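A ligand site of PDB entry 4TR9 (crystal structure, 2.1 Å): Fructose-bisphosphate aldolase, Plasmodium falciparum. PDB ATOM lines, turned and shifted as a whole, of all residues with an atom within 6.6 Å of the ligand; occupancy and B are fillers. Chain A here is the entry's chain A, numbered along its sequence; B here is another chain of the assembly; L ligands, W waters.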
ATOM      1  N   ALA A  38       3.219  15.209 -30.348  1.00  0.00           N
ATOM      2  CA  ALA A  38       4.227  14.538 -29.545  1.00  0.00           C
ATOM      3  C   ALA A  38       4.373  15.193 -28.173  1.00  0.00           C
ATOM      4  O   ALA A  38       5.149  16.132 -27.995  1.00  0.00           O
ATOM      5  CB  ALA A  38       5.572  14.540 -30.271  1.00  0.00           C
ATOM      6  N   ALA A  39       3.607  14.689 -27.201  1.00  0.00           N
ATOM      7  CA  ALA A  39       3.664  15.210 -25.845  1.00  0.00           C
ATOM      8  C   ALA A  39       4.145  14.150 -24.860  1.00  0.00           C
ATOM      9  O   ALA A  39       3.604  14.016 -23.763  1.00  0.00           O
ATOM     10  CB  ALA A  39       2.303  15.741 -25.432  1.00  0.00           C
ATOM     11  N   ASP A  40       5.153  13.384 -25.273  1.00  0.00           N
ATOM     12  CA  ASP A  40       5.674  12.303 -24.447  1.00  0.00           C
ATOM     13  C   ASP A  40       7.061  12.613 -23.900  1.00  0.00           C
ATOM     14  O   ASP A  40       7.957  11.767 -23.914  1.00  0.00           O
ATOM     15  CB  ASP A  40       5.715  10.998 -25.250  1.00  0.00           C
ATOM     16  CG  ASP A  40       6.393  11.168 -26.592  1.00  0.00           C
ATOM     17  OD1 ASP A  40       6.293  12.266 -27.177  1.00  0.00           O
ATOM     18  OD2 ASP A  40       7.020  10.190 -27.069  1.00  0.00           O
ATOM     19  N   GLU A  41       7.240  13.849 -23.422  1.00  0.00           N
ATOM     20  CA  GLU A  41       8.503  14.251 -22.826  1.00  0.00           C
ATOM     21  C   GLU A  41       8.714  13.587 -21.473  1.00  0.00           C
ATOM     22  O   GLU A  41       7.789  13.500 -20.673  1.00  0.00           O
ATOM     23  CB  GLU A  41       8.574  15.776 -22.671  1.00  0.00           C
ATOM     24  CG  GLU A  41       8.471  16.554 -23.978  1.00  0.00           C
ATOM     25  CD  GLU A  41       7.042  16.730 -24.459  1.00  0.00           C
ATOM     26  OE1 GLU A  41       6.117  16.443 -23.685  1.00  0.00           O
ATOM     27  OE2 GLU A  41       6.859  17.165 -25.611  1.00  0.00           O
ATOM     28  N   SER A  42       9.935  13.119 -21.227  1.00  0.00           N
ATOM     29  CA  SER A  42      10.258  12.500 -19.948  1.00  0.00           C
ATOM     30  C   SER A  42      10.345  13.559 -18.854  1.00  0.00           C
ATOM     31  O   SER A  42      10.191  14.754 -19.117  1.00  0.00           O
ATOM     32  CB  SER A  42      11.575  11.727 -20.032  1.00  0.00           C
ATOM     33  OG  SER A  42      12.653  12.585 -20.338  1.00  0.00           O
ATOM     34  N   GLN A  44      12.953  14.576 -17.000  1.00  0.00           N
ATOM     35  CA  GLN A  44      14.107  15.460 -17.175  1.00  0.00           C
ATOM     36  C   GLN A  44      13.986  16.268 -18.460  1.00  0.00           C
ATOM     37  O   GLN A  44      14.607  17.320 -18.607  1.00  0.00           O
ATOM     38  CB  GLN A  44      15.406  14.655 -17.184  1.00  0.00           C
ATOM     39  CG  GLN A  44      15.510  13.655 -18.325  1.00  0.00           C
ATOM     40  CD  GLN A  44      16.833  12.904 -18.322  1.00  0.00           C
ATOM     41  OE1 GLN A  44      17.611  13.006 -17.380  1.00  0.00           O
ATOM     42  NE2 GLN A  44      17.081  12.146 -19.391  1.00  0.00           N
ATOM     43  N   THR A  45      13.178  15.782 -19.397  1.00  0.00           N
ATOM     44  CA  THR A  45      12.974  16.471 -20.674  1.00  0.00           C
ATOM     45  C   THR A  45      11.983  17.611 -20.517  1.00  0.00           C
ATOM     46  O   THR A  45      12.221  18.726 -20.979  1.00  0.00           O
ATOM     47  CB  THR A  45      12.462  15.502 -21.760  1.00  0.00           C
ATOM     48  OG1 THR A  45      13.390  14.429 -21.921  1.00  0.00           O
ATOM     49  CG2 THR A  45      12.305  16.234 -23.083  1.00  0.00           C
ATOM     50  N   LYS A  48      13.360  20.854 -18.564  1.00  0.00           N
ATOM     51  CA  LYS A  48      14.059  21.908 -19.282  1.00  0.00           C
ATOM     52  C   LYS A  48      13.088  22.848 -19.990  1.00  0.00           C
ATOM     53  O   LYS A  48      13.450  23.960 -20.377  1.00  0.00           O
ATOM     54  CB  LYS A  48      15.038  21.307 -20.295  1.00  0.00           C
ATOM     55  CG  LYS A  48      16.086  20.398 -19.660  1.00  0.00           C
ATOM     56  CD  LYS A  48      17.064  19.879 -20.704  1.00  0.00           C
ATOM     57  CE  LYS A  48      18.099  18.952 -20.063  1.00  0.00           C
ATOM     58  NZ  LYS A  48      18.859  19.640 -18.985  1.00  0.00           N
ATOM     59  N   ARG A  49      11.851  22.391 -20.167  1.00  0.00           N
ATOM     60  CA  ARG A  49      10.807  23.223 -20.750  1.00  0.00           C
ATOM     61  C   ARG A  49      10.228  24.169 -19.713  1.00  0.00           C
ATOM     62  O   ARG A  49      10.045  25.358 -19.973  1.00  0.00           O
ATOM     63  CB  ARG A  49       9.699  22.353 -21.346  1.00  0.00           C
ATOM     64  CG  ARG A  49      10.192  21.369 -22.396  1.00  0.00           C
ATOM     65  CD  ARG A  49      10.849  22.092 -23.556  1.00  0.00           C
ATOM     66  NE  ARG A  49      11.792  21.237 -24.261  1.00  0.00           N
ATOM     67  CZ  ARG A  49      13.108  21.259 -24.065  1.00  0.00           C
ATOM     68  NH1 ARG A  49      13.891  20.441 -24.746  1.00  0.00           N
ATOM     69  NH2 ARG A  49      13.633  22.089 -23.180  1.00  0.00           N
ATOM     70  N   ILE A  83       0.912  11.311 -28.501  1.00  0.00           N
ATOM     71  CA  ILE A  83       1.823  10.385 -27.834  1.00  0.00           C
ATOM     72  C   ILE A  83       2.055  10.819 -26.392  1.00  0.00           C
ATOM     73  O   ILE A  83       2.421  11.955 -26.137  1.00  0.00           O
ATOM     74  CB  ILE A  83       3.180  10.296 -28.570  1.00  0.00           C
ATOM     75  CG1 ILE A  83       2.952  10.194 -30.079  1.00  0.00           C
ATOM     76  CG2 ILE A  83       3.982   9.113 -28.051  1.00  0.00           C
ATOM     77  CD1 ILE A  83       4.235  10.183 -30.882  1.00  0.00           C
ATOM     78  N   LYS A 113       4.980   6.355 -25.376  1.00  0.00           N
ATOM     79  CA  LYS A 113       6.423   6.198 -25.558  1.00  0.00           C
ATOM     80  C   LYS A 113       6.899   4.973 -24.771  1.00  0.00           C
ATOM     81  O   LYS A 113       6.698   4.894 -23.557  1.00  0.00           O
ATOM     82  CB  LYS A 113       7.163   7.453 -25.099  1.00  0.00           C
ATOM     83  CG  LYS A 113       8.671   7.335 -25.078  1.00  0.00           C
ATOM     84  CD  LYS A 113       9.277   8.556 -24.393  1.00  0.00           C
ATOM     85  CE  LYS A 113      10.791   8.509 -24.423  1.00  0.00           C
ATOM     86  NZ  LYS A 113      11.308   8.613 -25.817  1.00  0.00           N
ATOM     87  N   ASP A 115      10.174   3.481 -25.235  1.00  0.00           N
ATOM     88  CA  ASP A 115      11.625   3.356 -25.185  1.00  0.00           C
ATOM     89  C   ASP A 115      12.162   3.797 -23.825  1.00  0.00           C
ATOM     90  O   ASP A 115      11.582   4.660 -23.169  1.00  0.00           O
ATOM     91  CB  ASP A 115      12.277   4.147 -26.317  1.00  0.00           C
ATOM     92  CG  ASP A 115      12.171   5.647 -26.139  1.00  0.00           C
ATOM     93  OD1 ASP A 115      13.029   6.223 -25.437  1.00  0.00           O
ATOM     94  OD2 ASP A 115      11.227   6.238 -26.704  1.00  0.00           O
ATOM     95  N   LYS A 152       5.617   4.346 -29.608  1.00  0.00           N
ATOM     96  CA  LYS A 152       6.733   5.066 -30.224  1.00  0.00           C
ATOM     97  C   LYS A 152       8.069   4.628 -29.632  1.00  0.00           C
ATOM     98  O   LYS A 152       8.150   4.222 -28.476  1.00  0.00           O
ATOM     99  CB  LYS A 152       6.546   6.570 -30.052  1.00  0.00           C
ATOM    100  CG  LYS A 152       7.241   7.401 -31.118  1.00  0.00           C
ATOM    101  CD  LYS A 152       7.877   8.635 -30.508  1.00  0.00           C
ATOM    102  CE  LYS A 152       8.893   8.248 -29.459  1.00  0.00           C
ATOM    103  NZ  LYS A 152       9.546   9.434 -28.851  1.00  0.00           N
ATOM    104  N   ARG A 154      12.192   5.916 -30.132  1.00  0.00           N
ATOM    105  CA  ARG A 154      13.116   6.851 -30.768  1.00  0.00           C
ATOM    106  C   ARG A 154      14.567   6.360 -30.767  1.00  0.00           C
ATOM    107  O   ARG A 154      15.126   6.050 -29.718  1.00  0.00           O
ATOM    108  CB  ARG A 154      13.044   8.218 -30.077  1.00  0.00           C
ATOM    109  CG  ARG A 154      14.064   9.226 -30.581  1.00  0.00           C
ATOM    110  CD  ARG A 154      13.843  10.580 -29.932  1.00  0.00           C
ATOM    111  NE  ARG A 154      14.848  11.563 -30.349  1.00  0.00           N
ATOM    112  CZ  ARG A 154      15.934  11.867 -29.638  1.00  0.00           C
ATOM    113  NH1 ARG A 154      16.780  12.770 -30.098  1.00  0.00           N
ATOM    114  NH2 ARG A 154      16.167  11.254 -28.489  1.00  0.00           N
ATOM    115  N   GLU A 195      10.991   5.328 -35.462  1.00  0.00           N
ATOM    116  CA  GLU A 195      11.684   6.611 -35.502  1.00  0.00           C
ATOM    117  C   GLU A 195      13.207   6.451 -35.545  1.00  0.00           C
ATOM    118  O   GLU A 195      13.851   6.392 -34.497  1.00  0.00           O
ATOM    119  CB  GLU A 195      11.283   7.469 -34.296  1.00  0.00           C
ATOM    120  CG  GLU A 195      11.893   8.868 -34.296  1.00  0.00           C
ATOM    121  CD  GLU A 195      11.511   9.671 -33.063  1.00  0.00           C
ATOM    122  OE1 GLU A 195      10.661   9.189 -32.290  1.00  0.00           O
ATOM    123  OE2 GLU A 195      12.077  10.768 -32.875  1.00  0.00           O
ATOM    124  N   GLU A 197      15.678   8.653 -36.133  1.00  0.00           N
ATOM    125  CA  GLU A 197      16.029  10.060 -36.267  1.00  0.00           C
ATOM    126  C   GLU A 197      17.513  10.269 -36.547  1.00  0.00           C
ATOM    127  O   GLU A 197      18.372   9.837 -35.773  1.00  0.00           O
ATOM    128  CB  GLU A 197      15.633  10.843 -35.019  1.00  0.00           C
ATOM    129  CG  GLU A 197      16.014  12.323 -35.085  1.00  0.00           C
ATOM    130  CD  GLU A 197      15.706  13.064 -33.804  1.00  0.00           C
ATOM    131  OE1 GLU A 197      15.227  12.426 -32.844  1.00  0.00           O
ATOM    132  OE2 GLU A 197      15.951  14.288 -33.767  1.00  0.00           O
ATOM    133  N   LEU A 199      20.234  13.096 -36.652  1.00  0.00           N
ATOM    134  CA  LEU A 199      20.473  14.455 -36.187  1.00  0.00           C
ATOM    135  C   LEU A 199      20.993  15.361 -37.289  1.00  0.00           C
ATOM    136  O   LEU A 199      21.815  14.934 -38.116  1.00  0.00           O
ATOM    137  CB  LEU A 199      21.444  14.453 -35.004  1.00  0.00           C
ATOM    138  CG  LEU A 199      20.985  13.713 -33.755  1.00  0.00           C
ATOM    139  CD1 LEU A 199      22.012  13.853 -32.645  1.00  0.00           C
ATOM    140  CD2 LEU A 199      19.628  14.219 -33.303  1.00  0.00           C
ATOM    141  N   LYS A 237       8.709   7.658 -38.586  1.00  0.00           N
ATOM    142  CA  LYS A 237       8.994   8.985 -38.064  1.00  0.00           C
ATOM    143  C   LYS A 237      10.450   9.358 -38.297  1.00  0.00           C
ATOM    144  O   LYS A 237      11.272   9.269 -37.392  1.00  0.00           O
ATOM    145  CB  LYS A 237       8.653   9.069 -36.569  1.00  0.00           C
ATOM    146  CG  LYS A 237       8.761  10.468 -35.981  1.00  0.00           C
ATOM    147  CD  LYS A 237       8.300  10.494 -34.527  1.00  0.00           C
ATOM    148  CE  LYS A 237       8.410  11.894 -33.949  1.00  0.00           C
ATOM    149  NZ  LYS A 237       7.897  11.957 -32.552  1.00  0.00           N
ATOM    150  N   LEU A 278       9.337  14.547 -37.864  1.00  0.00           N
ATOM    151  CA  LEU A 278       9.644  15.157 -36.580  1.00  0.00           C
ATOM    152  C   LEU A 278      10.207  16.558 -36.795  1.00  0.00           C
ATOM    153  O   LEU A 278      10.971  16.796 -37.730  1.00  0.00           O
ATOM    154  CB  LEU A 278      10.619  14.291 -35.788  1.00  0.00           C
ATOM    155  CG  LEU A 278      11.954  13.899 -36.435  1.00  0.00           C
ATOM    156  CD1 LEU A 278      13.059  14.886 -36.092  1.00  0.00           C
ATOM    157  CD2 LEU A 278      12.343  12.480 -36.041  1.00  0.00           C
ATOM    158  N   SER A 307       4.559  14.601 -36.814  1.00  0.00           N
ATOM    159  CA  SER A 307       4.499  14.131 -35.438  1.00  0.00           C
ATOM    160  C   SER A 307       5.264  15.115 -34.567  1.00  0.00           C
ATOM    161  O   SER A 307       6.251  14.764 -33.911  1.00  0.00           O
ATOM    162  CB  SER A 307       5.084  12.726 -35.301  1.00  0.00           C
ATOM    163  OG  SER A 307       5.034  12.283 -33.961  1.00  0.00           O
ATOM    164  N   ASP B   1      17.272  19.062 -28.959  1.00  0.00           N
ATOM    165  CA  ASP B   1      16.470  18.624 -30.094  1.00  0.00           C
ATOM    166  C   ASP B   1      14.973  18.774 -29.800  1.00  0.00           C
ATOM    167  O   ASP B   1      14.291  19.578 -30.428  1.00  0.00           O
ATOM    168  CB  ASP B   1      16.799  17.173 -30.447  1.00  0.00           C
ATOM    169  CG  ASP B   1      16.170  16.729 -31.754  1.00  0.00           C
ATOM    170  OD1 ASP B   1      16.816  16.918 -32.812  1.00  0.00           O
ATOM    171  OD2 ASP B   1      15.034  16.204 -31.733  1.00  0.00           O
ATOM    172  N   TRP B   2      14.484  17.996 -28.839  1.00  0.00           N
ATOM    173  CA  TRP B   2      13.081  18.043 -28.386  1.00  0.00           C
ATOM    174  C   TRP B   2      12.077  17.741 -29.492  1.00  0.00           C
ATOM    175  O   TRP B   2      11.676  18.637 -30.236  1.00  0.00           O
ATOM    176  CB  TRP B   2      12.767  19.400 -27.755  1.00  0.00           C
ATOM    177  CG  TRP B   2      11.396  19.468 -27.137  1.00  0.00           C
ATOM    178  CD1 TRP B   2      10.694  18.430 -26.614  1.00  0.00           C
ATOM    179  CD2 TRP B   2      10.570  20.636 -26.984  1.00  0.00           C
ATOM    180  NE1 TRP B   2       9.471  18.869 -26.144  1.00  0.00           N
ATOM    181  CE2 TRP B   2       9.381  20.219 -26.364  1.00  0.00           C
ATOM    182  CE3 TRP B   2      10.734  21.985 -27.317  1.00  0.00           C
ATOM    183  CZ2 TRP B   2       8.346  21.105 -26.064  1.00  0.00           C
ATOM    184  CZ3 TRP B   2       9.703  22.857 -27.019  1.00  0.00           C
ATOM    185  CH2 TRP B   2       8.525  22.421 -26.399  1.00  0.00           C
ATOM    186  N   ASN B   3      11.657  16.484 -29.569  1.00  0.00           N
ATOM    187  CA  ASN B   3      10.650  16.023 -30.532  1.00  0.00           C
ATOM    188  C   ASN B   3      11.019  16.327 -31.991  1.00  0.00           C
ATOM    189  O   ASN B   3      12.189  16.511 -32.328  1.00  0.00           O
ATOM    190  CB  ASN B   3       9.288  16.643 -30.220  1.00  0.00           C
ATOM    191  CG  ASN B   3       8.916  16.533 -28.747  1.00  0.00           C
ATOM    192  OD1 ASN B   3       8.331  17.446 -28.177  1.00  0.00           O
ATOM    193  ND2 ASN B   3       9.273  15.407 -28.135  1.00  0.00           N
ATOM    194  OXT ASN B   3      10.139  16.392 -32.849  1.00  0.00           O
HETATM  195  N1  LIG L   1      15.239  13.559 -25.078  1.00  0.00           N
HETATM  196  C1  LIG L   1      15.940  14.674 -25.664  1.00  0.00           C
HETATM  197  C2  LIG L   1      17.482  14.549 -23.703  1.00  0.00           C
HETATM  198  C3  LIG L   1      19.775  15.242 -23.828  1.00  0.00           C
HETATM  199  C4  LIG L   1      18.392  15.406 -25.772  1.00  0.00           C
HETATM  200  C5  LIG L   1      12.088  12.881 -27.943  1.00  0.00           C
HETATM  201  C6  LIG L   1      11.080  12.724 -28.898  1.00  0.00           C
HETATM  202  O1  LIG L   1      11.351  12.877 -30.284  1.00  0.00           O
HETATM  203  C7  LIG L   1       9.792  12.430 -28.497  1.00  0.00           C
HETATM  204  C8  LIG L   1       9.505  12.284 -27.144  1.00  0.00           C
HETATM  205  C9  LIG L   1      10.494  12.429 -26.195  1.00  0.00           C
HETATM  206  O2  LIG L   1       8.751  12.279 -29.437  1.00  0.00           O
HETATM  207  C10 LIG L   1      11.783  12.724 -26.596  1.00  0.00           C
HETATM  208  C11 LIG L   1      12.855  12.890 -25.514  1.00  0.00           C
HETATM  209  O3  LIG L   1      12.582  12.662 -24.344  1.00  0.00           O
HETATM  210  N2  LIG L   1      14.163  13.335 -25.932  1.00  0.00           N
HETATM  211  C12 LIG L   1      17.321  14.881 -25.029  1.00  0.00           C
HETATM  212  C13 LIG L   1      18.716  14.733 -23.090  1.00  0.00           C
HETATM  213 CL1  LIG L   1      21.310  15.452 -23.038  1.00  0.00          CL
HETATM  214  C14 LIG L   1      19.621  15.583 -25.161  1.00  0.00           C
HETATM  215 CL2  LIG L   1      18.212  15.831 -27.449  1.00  0.00          CL
HETATM  216  O   HOH W   1      12.899  13.811 -31.946  1.00  0.00           O
HETATM  217  O   HOH W   2       7.194  14.568 -27.009  1.00  0.00           O
HETATM  218  O   HOH W   3      12.095  15.733 -26.319  1.00  0.00           O
HETATM  219  O   HOH W   4      14.390  14.933 -28.802  1.00  0.00           O
HETATM  220  O   HOH W   5      18.888  12.627 -27.985  1.00  0.00           O
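OD2 of Asp 40 is in salt-bridge range of NZ of Lys 152 (3.2 Å).
OE2 of Glu 41 lies close to OD1 of Asn 3 of chain B (3.0 Å).
The side-chain amide oxygen (OD1) of Asn 3 of chain B lies within hydrogen-bond range of the indole nitrogen (NE1) of Trp 2 of chain B (2.7 Å).
OG1 of Thr 45 lies within hydrogen-bond range of OG of Ser 42.
NZ of Lys 237 lies within salt-bridge range of OE1 of Glu 195 (3.9 Å).
The side-chain amino group of Lys 237 is in hydrogen-bond range of the side-chain hydroxyl of Ser 307 (3.2 Å).
The side-chain carboxylate (OE2) of Glu 195 lies within salt-bridge range of the guanidinium group (NE) of Arg 154 (3.8 Å).
The side-chain carboxylate (OE1) of Glu 197 lies within salt-bridge range of the guanidinium group (NE) of Arg 154.
Ala 38 touches the ligand.
Lys 113 touches the ligand (NZ to C9, 3.9 Å).
Arg 154 touches the ligand (CD to O1, 3.4 Å).
Asp 1 of chain B touches the ligand.
Hydrophobic or aromatic side chains within 4 Å of the ligand: Ala 38.
Of the 23 residues printed, 10 come within 4 Å of the ligand.
The nearest printed residue that does not touch the ligand is Ser 42 (4.01 Å).
NZ of Lys 152 is in hydrogen-bond range of O2 of the ligand, 3.0 Å away.
An oxygen (O2) of the ligand lies close to the side-chain amide nitrogen (ND2) of Asn 3 of chain B (3.4 Å).
The side-chain hydroxyl (OG1) of Thr 45 is in hydrogen-bond range of an oxygen (O3) of the ligand.
The side-chain carboxylate (OD1) of Asp 40 lies close to an oxygen (O2) of the ligand (3.3 Å).
The side-chain amino group of Lys 237 lies within hydrogen-bond range of an oxygen (O2) of the ligand, at 3.2 Å.
An oxygen (O1) of the ligand is in hydrogen-bond range of the side-chain carboxylate (OE2) of Glu 195 (3.4 Å).
Water W3 lies within hydrogen-bond range of N2 of the ligand (3.2 Å) and N of Asn 3 of chain B (3.4 Å).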
